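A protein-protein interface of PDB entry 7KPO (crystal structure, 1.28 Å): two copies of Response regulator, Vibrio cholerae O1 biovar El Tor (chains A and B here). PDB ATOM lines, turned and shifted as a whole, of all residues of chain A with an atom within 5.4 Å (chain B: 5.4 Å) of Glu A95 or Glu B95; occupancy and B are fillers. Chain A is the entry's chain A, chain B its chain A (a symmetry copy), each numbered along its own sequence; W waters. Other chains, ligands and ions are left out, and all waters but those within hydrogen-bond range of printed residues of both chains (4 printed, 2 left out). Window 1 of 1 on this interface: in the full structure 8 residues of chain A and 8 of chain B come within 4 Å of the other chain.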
ATOM      1  N   LEU A  81      23.502 -13.379   4.203  1.00  0.00           N
ATOM      2  CA  LEU A  81      22.275 -12.628   3.811  1.00  0.00           C
ATOM      3  C   LEU A  81      22.132 -12.606   2.276  1.00  0.00           C
ATOM      4  O   LEU A  81      20.986 -12.594   1.781  1.00  0.00           O
ATOM      5  CB  LEU A  81      22.335 -11.221   4.417  1.00  0.00           C
ATOM      6  CG  LEU A  81      22.178 -11.153   5.938  1.00  0.00           C
ATOM      7  CD1 LEU A  81      22.481  -9.754   6.456  1.00  0.00           C
ATOM      8  CD2 LEU A  81      20.782 -11.596   6.366  1.00  0.00           C
ATOM      9  N   LYS A  85      17.556 -15.644   1.806  1.00  0.00           N
ATOM     10  CA  LYS A  85      16.636 -14.480   1.705  1.00  0.00           C
ATOM     11  C   LYS A  85      15.395 -14.588   2.592  1.00  0.00           C
ATOM     12  O   LYS A  85      14.802 -13.529   2.844  1.00  0.00           O
ATOM     13  CB  LYS A  85      16.192 -14.339   0.248  1.00  0.00           C
ATOM     14  CG  LYS A  85      17.305 -14.045  -0.743  1.00  0.00           C
ATOM     15  CD  LYS A  85      18.084 -12.810  -0.373  1.00  0.00           C
ATOM     16  CE  LYS A  85      19.042 -12.350  -1.446  1.00  0.00           C
ATOM     17  NZ  LYS A  85      19.895 -11.250  -0.941  1.00  0.00           N
ATOM     18  N   ALA A  87      12.566 -14.014   4.566  1.00  0.00           N
ATOM     19  CA  ALA A  87      12.233 -12.857   5.419  1.00  0.00           C
ATOM     20  C   ALA A  87      11.571 -13.342   6.703  1.00  0.00           C
ATOM     21  O   ALA A  87      10.840 -14.348   6.681  1.00  0.00           O
ATOM     22  CB  ALA A  87      11.339 -11.903   4.672  1.00  0.00           C
ATOM     23  N   GLY A  88      11.844 -12.646   7.795  1.00  0.00           N
ATOM     24  CA  GLY A  88      11.238 -13.030   9.072  1.00  0.00           C
ATOM     25  C   GLY A  88      12.070 -12.512  10.229  1.00  0.00           C
ATOM     26  O   GLY A  88      13.117 -11.897  10.023  1.00  0.00           O
ATOM     27  N   ARG A  91      15.940 -13.382  10.266  1.00  0.00           N
ATOM     28  CA  ARG A  91      16.753 -12.574   9.327  1.00  0.00           C
ATOM     29  C   ARG A  91      16.862 -11.130   9.828  1.00  0.00           C
ATOM     30  O   ARG A  91      17.965 -10.561   9.788  1.00  0.00           O
ATOM     31  CB  ARG A  91      16.135 -12.600   7.931  1.00  0.00           C
ATOM     32  CG  ARG A  91      17.092 -12.103   6.863  1.00  0.00           C
ATOM     33  CD  ARG A  91      16.482 -12.214   5.486  1.00  0.00           C
ATOM     34  NE  ARG A  91      17.510 -12.243   4.448  1.00  0.00           N
ATOM     35  CZ  ARG A  91      18.016 -11.172   3.850  1.00  0.00           C
ATOM     36  NH1 ARG A  91      17.596  -9.963   4.178  1.00  0.00           N
ATOM     37  NH2 ARG A  91      18.946 -11.309   2.924  1.00  0.00           N
ATOM     38  N   THR A  92      15.754 -10.559  10.286  1.00  0.00           N
ATOM     39  CA  THR A  92      15.762  -9.159  10.777  1.00  0.00           C
ATOM     40  C   THR A  92      16.779  -9.031  11.919  1.00  0.00           C
ATOM     41  O   THR A  92      17.502  -8.019  11.972  1.00  0.00           O
ATOM     42  CB  THR A  92      14.348  -8.750  11.193  1.00  0.00           C
ATOM     43  OG1 THR A  92      13.521  -8.779  10.026  1.00  0.00           O
ATOM     44  CG2 THR A  92      14.303  -7.385  11.841  1.00  0.00           C
ATOM     45  N   HIS A  93      16.840 -10.029  12.795  1.00  0.00           N
ATOM     46  CA  HIS A  93      17.785  -9.982  13.940  1.00  0.00           C
ATOM     47  C   HIS A  93      19.224  -9.891  13.431  1.00  0.00           C
ATOM     48  O   HIS A  93      20.001  -9.100  13.981  1.00  0.00           O
ATOM     49  CB  HIS A  93      17.562 -11.201  14.837  1.00  0.00           C
ATOM     50  CG  HIS A  93      18.534 -11.304  15.957  1.00  0.00           C
ATOM     51  ND1 HIS A  93      18.491 -10.464  17.047  1.00  0.00           N
ATOM     52  CD2 HIS A  93      19.555 -12.156  16.176  1.00  0.00           C
ATOM     53  CE1 HIS A  93      19.458 -10.786  17.884  1.00  0.00           C
ATOM     54  NE2 HIS A  93      20.116 -11.822  17.376  1.00  0.00           N
ATOM     55  N   ILE A  94      19.561 -10.670  12.410  1.00  0.00           N
ATOM     56  CA  ILE A  94      20.940 -10.640  11.842  1.00  0.00           C
ATOM     57  C   ILE A  94      21.199  -9.251  11.248  1.00  0.00           C
ATOM     58  O   ILE A  94      22.285  -8.695  11.472  1.00  0.00           O
ATOM     59  CB  ILE A  94      21.121 -11.764  10.812  1.00  0.00           C
ATOM     60  CG1 ILE A  94      20.998 -13.134  11.484  1.00  0.00           C
ATOM     61  CG2 ILE A  94      22.448 -11.611  10.091  1.00  0.00           C
ATOM     62  CD1 ILE A  94      20.673 -14.259  10.540  1.00  0.00           C
ATOM     63  N   GLU A  95      20.238  -8.713  10.500  1.00  0.00           N
ATOM     64  CA  GLU A  95      20.420  -7.370   9.895  1.00  0.00           C
ATOM     65  C   GLU A  95      20.633  -6.324  10.984  1.00  0.00           C
ATOM     66  O   GLU A  95      21.467  -5.434  10.835  1.00  0.00           O
ATOM     67  CB  GLU A  95      19.204  -6.973   9.063  1.00  0.00           C
ATOM     68  CG  GLU A  95      18.920  -7.900   7.902  1.00  0.00           C
ATOM     69  CD  GLU A  95      17.721  -7.443   7.096  1.00  0.00           C
ATOM     70  OE1 GLU A  95      17.608  -6.221   6.853  1.00  0.00           O
ATOM     71  OE2 GLU A  95      16.879  -8.293   6.763  1.00  0.00           O
ATOM     72  N   MET A  96      19.866  -6.427  12.074  1.00  0.00           N
ATOM     73  CA  MET A  96      19.965  -5.469  13.162  1.00  0.00           C
ATOM     74  C   MET A  96      21.327  -5.584  13.849  1.00  0.00           C
ATOM     75  O   MET A  96      21.934  -4.566  14.185  1.00  0.00           O
ATOM     76  CB  MET A  96      18.789  -5.667  14.122  1.00  0.00           C
ATOM     77  CG  MET A  96      17.438  -5.304  13.518  1.00  0.00           C
ATOM     78  SD  MET A  96      17.189  -3.380  13.317  1.00  0.00           S
ATOM     79  CE  MET A  96      17.010  -2.717  15.145  1.00  0.00           C
ATOM     80  N   GLN A  97      21.823  -6.810  14.045  1.00  0.00           N
ATOM     81  CA  GLN A  97      23.115  -6.989  14.696  1.00  0.00           C
ATOM     82  C   GLN A  97      24.226  -6.478  13.762  1.00  0.00           C
ATOM     83  O   GLN A  97      25.204  -5.896  14.275  1.00  0.00           O
ATOM     84  CB  GLN A  97      23.300  -8.448  15.127  1.00  0.00           C
ATOM     85  CG  GLN A  97      22.326  -8.895  16.215  1.00  0.00           C
ATOM     86  CD  GLN A  97      22.658  -8.355  17.586  1.00  0.00           C
ATOM     87  OE1 GLN A  97      23.747  -8.569  18.106  1.00  0.00           O
ATOM     88  NE2 GLN A  97      21.690  -7.716  18.219  1.00  0.00           N
ATOM     89  N   ARG A  98      24.080  -6.689  12.450  1.00  0.00           N
ATOM     90  CA  ARG A  98      25.080  -6.174  11.473  1.00  0.00           C
ATOM     91  C   ARG A  98      25.143  -4.647  11.606  1.00  0.00           C
ATOM     92  O   ARG A  98      26.250  -4.094  11.681  1.00  0.00           O
ATOM     93  CB  ARG A  98      24.701  -6.553  10.034  1.00  0.00           C
ATOM     94  CG  ARG A  98      25.555  -5.884   8.959  1.00  0.00           C
ATOM     95  CD  ARG A  98      25.257  -6.334   7.535  1.00  0.00           C
ATOM     96  NE  ARG A  98      23.893  -6.107   7.069  1.00  0.00           N
ATOM     97  CZ  ARG A  98      23.436  -6.432   5.857  1.00  0.00           C
ATOM     98  NH1 ARG A  98      24.230  -7.007   4.964  1.00  0.00           N
ATOM     99  NH2 ARG A  98      22.180  -6.183   5.542  1.00  0.00           N
ATOM    100  N   ASP A  99      23.985  -3.989  11.626  1.00  0.00           N
ATOM    101  CA  ASP A  99      23.969  -2.506  11.729  1.00  0.00           C
ATOM    102  C   ASP A  99      24.575  -2.056  13.058  1.00  0.00           C
ATOM    103  O   ASP A  99      25.305  -1.057  13.077  1.00  0.00           O
ATOM    104  CB  ASP A  99      22.553  -1.952  11.577  1.00  0.00           C
ATOM    105  CG  ASP A  99      22.063  -1.916  10.142  1.00  0.00           C
ATOM    106  OD1 ASP A  99      22.773  -2.460   9.267  1.00  0.00           O
ATOM    107  OD2 ASP A  99      20.996  -1.314   9.906  1.00  0.00           O
ATOM    108  N   LYS A 100      24.303  -2.796  14.130  1.00  0.00           N
ATOM    109  CA  LYS A 100      24.849  -2.443  15.466  1.00  0.00           C
ATOM    110  C   LYS A 100      26.382  -2.499  15.396  1.00  0.00           C
ATOM    111  O   LYS A 100      27.038  -1.513  15.781  1.00  0.00           O
ATOM    112  CB  LYS A 100      24.267  -3.401  16.508  1.00  0.00           C
ATOM    113  CG  LYS A 100      24.576  -3.079  17.963  1.00  0.00           C
ATOM    114  CD  LYS A 100      23.973  -4.094  18.915  1.00  0.00           C
ATOM    115  CE  LYS A 100      24.171  -3.762  20.379  1.00  0.00           C
ATOM    116  NZ  LYS A 100      23.501  -2.492  20.745  1.00  0.00           N
ATOM    117  N   LEU B  81      16.756  -3.035  -2.223  1.00  0.00           N
ATOM    118  CA  LEU B  81      17.318  -3.717  -1.023  1.00  0.00           C
ATOM    119  C   LEU B  81      18.844  -3.882  -1.169  1.00  0.00           C
ATOM    120  O   LEU B  81      19.552  -3.848  -0.141  1.00  0.00           O
ATOM    121  CB  LEU B  81      16.598  -5.056  -0.826  1.00  0.00           C
ATOM    122  CG  LEU B  81      15.136  -4.957  -0.379  1.00  0.00           C
ATOM    123  CD1 LEU B  81      14.455  -6.317  -0.437  1.00  0.00           C
ATOM    124  CD2 LEU B  81      15.030  -4.359   1.020  1.00  0.00           C
ATOM    125  N   LYS B  85      20.453  -0.538   2.908  1.00  0.00           N
ATOM    126  CA  LYS B  85      20.636  -1.626   3.905  1.00  0.00           C
ATOM    127  C   LYS B  85      20.022  -1.327   5.273  1.00  0.00           C
ATOM    128  O   LYS B  85      19.805  -2.301   6.006  1.00  0.00           O
ATOM    129  CB  LYS B  85      22.135  -1.875   4.080  1.00  0.00           C
ATOM    130  CG  LYS B  85      22.861  -2.359   2.836  1.00  0.00           C
ATOM    131  CD  LYS B  85      22.243  -3.610   2.268  1.00  0.00           C
ATOM    132  CE  LYS B  85      23.065  -4.254   1.177  1.00  0.00           C
ATOM    133  NZ  LYS B  85      22.314  -5.365   0.550  1.00  0.00           N
ATOM    134  N   ALA B  87      18.601  -1.462   8.465  1.00  0.00           N
ATOM    135  CA  ALA B  87      17.738  -2.496   9.068  1.00  0.00           C
ATOM    136  C   ALA B  87      16.653  -1.831   9.907  1.00  0.00           C
ATOM    137  O   ALA B  87      16.902  -0.774  10.515  1.00  0.00           O
ATOM    138  CB  ALA B  87      18.563  -3.443   9.897  1.00  0.00           C
ATOM    139  N   GLY B  88      15.475  -2.433   9.916  1.00  0.00           N
ATOM    140  CA  GLY B  88      14.377  -1.874  10.708  1.00  0.00           C
ATOM    141  C   GLY B  88      13.041  -2.340  10.165  1.00  0.00           C
ATOM    142  O   GLY B  88      12.986  -3.057   9.166  1.00  0.00           O
ATOM    143  N   ARG B  91      12.317  -1.794   6.303  1.00  0.00           N
ATOM    144  CA  ARG B  91      13.009  -2.757   5.414  1.00  0.00           C
ATOM    145  C   ARG B  91      12.378  -4.147   5.547  1.00  0.00           C
ATOM    146  O   ARG B  91      12.153  -4.807   4.520  1.00  0.00           O
ATOM    147  CB  ARG B  91      14.496  -2.821   5.753  1.00  0.00           C
ATOM    148  CG  ARG B  91      15.310  -3.500   4.667  1.00  0.00           C
ATOM    149  CD  ARG B  91      16.785  -3.479   4.994  1.00  0.00           C
ATOM    150  NE  ARG B  91      17.599  -3.640   3.792  1.00  0.00           N
ATOM    151  CZ  ARG B  91      17.996  -4.804   3.293  1.00  0.00           C
ATOM    152  NH1 ARG B  91      17.658  -5.934   3.886  1.00  0.00           N
ATOM    153  NH2 ARG B  91      18.729  -4.838   2.196  1.00  0.00           N
ATOM    154  N   THR B  92      12.101  -4.576   6.773  1.00  0.00           N
ATOM    155  CA  THR B  92      11.503  -5.915   6.998  1.00  0.00           C
ATOM    156  C   THR B  92      10.177  -6.011   6.232  1.00  0.00           C
ATOM    157  O   THR B  92       9.899  -7.068   5.638  1.00  0.00           O
ATOM    158  CB  THR B  92      11.340  -6.161   8.500  1.00  0.00           C
ATOM    159  OG1 THR B  92      12.645  -6.181   9.086  1.00  0.00           O
ATOM    160  CG2 THR B  92      10.602  -7.446   8.802  1.00  0.00           C
ATOM    161  N   HIS B  93       9.391  -4.938   6.236  1.00  0.00           N
ATOM    162  CA  HIS B  93       8.084  -4.948   5.533  1.00  0.00           C
ATOM    163  C   HIS B  93       8.291  -5.209   4.041  1.00  0.00           C
ATOM    164  O   HIS B  93       7.536  -6.001   3.465  1.00  0.00           O
ATOM    165  CB  HIS B  93       7.353  -3.630   5.796  1.00  0.00           C
ATOM    166  CG  HIS B  93       6.076  -3.496   5.046  1.00  0.00           C
ATOM    167  ND1 HIS B  93       4.949  -4.215   5.378  1.00  0.00           N
ATOM    168  CD2 HIS B  93       5.731  -2.714   4.005  1.00  0.00           C
ATOM    169  CE1 HIS B  93       3.968  -3.892   4.558  1.00  0.00           C
ATOM    170  NE2 HIS B  93       4.422  -2.971   3.715  1.00  0.00           N
ATOM    171  N   ILE B  94       9.287  -4.567   3.441  1.00  0.00           N
ATOM    172  CA  ILE B  94       9.568  -4.768   1.991  1.00  0.00           C
ATOM    173  C   ILE B  94       9.983  -6.226   1.766  1.00  0.00           C
ATOM    174  O   ILE B  94       9.505  -6.845   0.803  1.00  0.00           O
ATOM    175  CB  ILE B  94      10.633  -3.772   1.507  1.00  0.00           C
ATOM    176  CG1 ILE B  94      10.114  -2.336   1.615  1.00  0.00           C
ATOM    177  CG2 ILE B  94      11.063  -4.107   0.090  1.00  0.00           C
ATOM    178  CD1 ILE B  94      11.193  -1.289   1.642  1.00  0.00           C
ATOM    179  N   GLU B  95      10.858  -6.755   2.618  1.00  0.00           N
ATOM    180  CA  GLU B  95      11.302  -8.163   2.462  1.00  0.00           C
ATOM    181  C   GLU B  95      10.110  -9.109   2.564  1.00  0.00           C
ATOM    182  O   GLU B  95      10.017 -10.075   1.811  1.00  0.00           O
ATOM    183  CB  GLU B  95      12.321  -8.540   3.534  1.00  0.00           C
ATOM    184  CG  GLU B  95      13.588  -7.715   3.500  1.00  0.00           C
ATOM    185  CD  GLU B  95      14.573  -8.149   4.567  1.00  0.00           C
ATOM    186  OE1 GLU B  95      14.731  -9.376   4.754  1.00  0.00           O
ATOM    187  OE2 GLU B  95      15.134  -7.270   5.240  1.00  0.00           O
ATOM    188  N   MET B  96       9.204  -8.833   3.508  1.00  0.00           N
ATOM    189  CA  MET B  96       8.042  -9.681   3.712  1.00  0.00           C
ATOM    190  C   MET B  96       7.113  -9.611   2.498  1.00  0.00           C
ATOM    191  O   MET B  96       6.581 -10.636   2.071  1.00  0.00           O
ATOM    192  CB  MET B  96       7.352  -9.291   5.021  1.00  0.00           C
ATOM    193  CG  MET B  96       8.176  -9.599   6.264  1.00  0.00           C
ATOM    194  SD  MET B  96       8.262 -11.507   6.664  1.00  0.00           S
ATOM    195  CE  MET B  96       6.457 -11.965   7.249  1.00  0.00           C
ATOM    196  N   GLN B  97       6.925  -8.417   1.927  1.00  0.00           N
ATOM    197  CA  GLN B  97       6.051  -8.281   0.769  1.00  0.00           C
ATOM    198  C   GLN B  97       6.703  -8.973  -0.441  1.00  0.00           C
ATOM    199  O   GLN B  97       5.961  -9.580  -1.241  1.00  0.00           O
ATOM    200  CB  GLN B  97       5.715  -6.806   0.522  1.00  0.00           C
ATOM    201  CG  GLN B  97       4.880  -6.173   1.633  1.00  0.00           C
ATOM    202  CD  GLN B  97       3.430  -6.597   1.620  1.00  0.00           C
ATOM    203  OE1 GLN B  97       2.726  -6.423   0.633  1.00  0.00           O
ATOM    204  NE2 GLN B  97       2.949  -7.086   2.750  1.00  0.00           N
ATOM    205  N   ARG B  98       8.031  -8.885  -0.565  1.00  0.00           N
ATOM    206  CA  ARG B  98       8.746  -9.576  -1.674  1.00  0.00           C
ATOM    207  C   ARG B  98       8.478 -11.082  -1.557  1.00  0.00           C
ATOM    208  O   ARG B  98       8.141 -11.715  -2.569  1.00  0.00           O
ATOM    209  CB  ARG B  98      10.258  -9.314  -1.612  1.00  0.00           C
ATOM    210  CG  ARG B  98      11.086 -10.156  -2.581  1.00  0.00           C
ATOM    211  CD  ARG B  98      12.573  -9.829  -2.603  1.00  0.00           C
ATOM    212  NE  ARG B  98      13.276  -9.988  -1.334  1.00  0.00           N
ATOM    213  CZ  ARG B  98      14.577  -9.750  -1.149  1.00  0.00           C
ATOM    214  NH1 ARG B  98      15.342  -9.336  -2.150  1.00  0.00           N
ATOM    215  NH2 ARG B  98      15.111  -9.924   0.045  1.00  0.00           N
ATOM    216  N   ASP B  99       8.631 -11.636  -0.355  1.00  0.00           N
ATOM    217  CA  ASP B  99       8.411 -13.095  -0.171  1.00  0.00           C
ATOM    218  C   ASP B  99       6.956 -13.457  -0.469  1.00  0.00           C
ATOM    219  O   ASP B  99       6.711 -14.507  -1.077  1.00  0.00           O
ATOM    220  CB  ASP B  99       8.791 -13.542   1.240  1.00  0.00           C
ATOM    221  CG  ASP B  99      10.286 -13.682   1.453  1.00  0.00           C
ATOM    222  OD1 ASP B  99      11.047 -13.290   0.540  1.00  0.00           O
ATOM    223  OD2 ASP B  99      10.676 -14.214   2.512  1.00  0.00           O
ATOM    224  N   LYS B 100       6.023 -12.593  -0.075  1.00  0.00           N
ATOM    225  CA  LYS B 100       4.582 -12.854  -0.323  1.00  0.00           C
ATOM    226  C   LYS B 100       4.353 -12.932  -1.839  1.00  0.00           C
ATOM    227  O   LYS B 100       3.767 -13.926  -2.309  1.00  0.00           O
ATOM    228  CB  LYS B 100       3.756 -11.751   0.345  1.00  0.00           C
ATOM    229  CG  LYS B 100       2.248 -11.949   0.349  1.00  0.00           C
ATOM    230  CD  LYS B 100       1.520 -10.797   1.015  1.00  0.00           C
ATOM    231  CE  LYS B 100       0.023 -10.995   1.129  1.00  0.00           C
ATOM    232  NZ  LYS B 100      -0.308 -12.161   1.981  1.00  0.00           N
HETATM  233  O   HOH W   1      19.300  -0.102  11.581  1.00  0.00           O
HETATM  234  O   HOH W   2       9.272 -15.107   4.605  1.00  0.00           O
HETATM  235  O   HOH W   3      15.378  -5.060   8.531  1.00  0.00           O
HETATM  236  O   HOH W   4      13.433 -10.173   7.365  1.00  0.00           O
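The side-chain carboxylate (OD2) of Asp A99 is in hydrogen-bond range of the backbone NH (N) of Ala B87, 2.8 Å away.
The side-chain carboxylate of Glu B95 is in salt-bridge range of the guanidinium group of Arg A91 (3.0 Å).
The guanidinium group (NH1) of Arg B91 is in salt-bridge range of the side-chain carboxylate (OE1) of Glu A95 (3.0 Å).
N of Ala A87 lies within hydrogen-bond range of OD2 of Asp B99, 2.8 Å away.
OE2 of Glu A95 sits close to OE2 of Glu B95, 2.5 Å away.
The side-chain hydroxyl (OG1) of Thr A92 sits at hydrogen-bond distance from the side-chain hydroxyl (OG1) of Thr B92 (2.9 Å).
The backbone carbonyl oxygen of Lys A85 lies close to the guanidinium group of Arg A91, 3.4 Å away.
The guanidinium group (NH2) of Arg A91 sits at hydrogen-bond distance from the backbone carbonyl oxygen (O) of Leu A81 (2.7 Å).
The side-chain hydroxyl (OG1) of Thr A92 lies within hydrogen-bond range of the backbone carbonyl oxygen (O) of Gly A88, at 3.1 Å.
NH1 of Arg A91 is in salt-bridge range of OE2 of Glu A95, at 3.2 Å.
O of Lys B85 lies close to NE of Arg B91 (3.4 Å).
The guanidinium group (NH1) of Arg B91 lies within salt-bridge range of the side-chain carboxylate (OE2) of Glu B95.
Among the printed residues, pairs that only touch across the chains: Ala A87 with Glu B95, Glu A95 with Ala B87, Met A96 with Ala B87, Ala A87 with Met B96, Met A96 with Gly B88 and Gly A88 with Met B96.
Of the printed residues of chain A, Glu B95 touches Ala A87, Arg A91 and Glu A95.
Printed residues of chain B within 4 Å of Arg A91: Glu B95 (3.0 Å).
Of the printed residues of chain B, Ala A87 touches Glu B95 (3.6 Å), Met B96 (3.7 Å) and Asp B99 (2.8 Å).
Printed residues of chain A within 4 Å of Arg B91: Glu A95 (3.0 Å).
Of the printed residues of chain B, Thr A92 touches Thr B92.
The nearest printed residue of chain B that does not touch Gly A88 is Thr B92 (5.3 Å).
Hydrophobic or aromatic side chains of chain A within 4 Å of the printed part of chain B: Ala A87 and Met A96.
Gly A88 touches Met B96, and with the chains exchanged Met A96 touches Gly B88.
Arg A91 touches Glu B95, and with the chains exchanged Glu A95 touches Arg B91.
Thr B92 touches its own counterpart, Thr A92.
Glu B95 touches its own counterpart, Glu A95.
Positions printed for both chains: 81, 85, 87, 88, 91, 92, 93, 94, 95, 96, 97, 98, 99 and 100.
Water W1 bridges OD2 of Asp A99 and O of Ala B87.
Water W2 lies within hydrogen-bond range of the side-chain carboxylate (OD2) of Asp B99 (2.7 Å) and the backbone carbonyl oxygen (O) of Ala A87 (2.7 Å).
Water W3 lies within hydrogen-bond range of the backbone NH of Gly B88 (3.0 Å), the side-chain hydroxyl of Thr B92 (3.0 Å) and the side-chain carboxylate of Glu A95 (3.0 Å).
Water W4 lies within hydrogen-bond range of N of Gly A88, OG1 of Thr A92 and OE1 of Glu B95.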
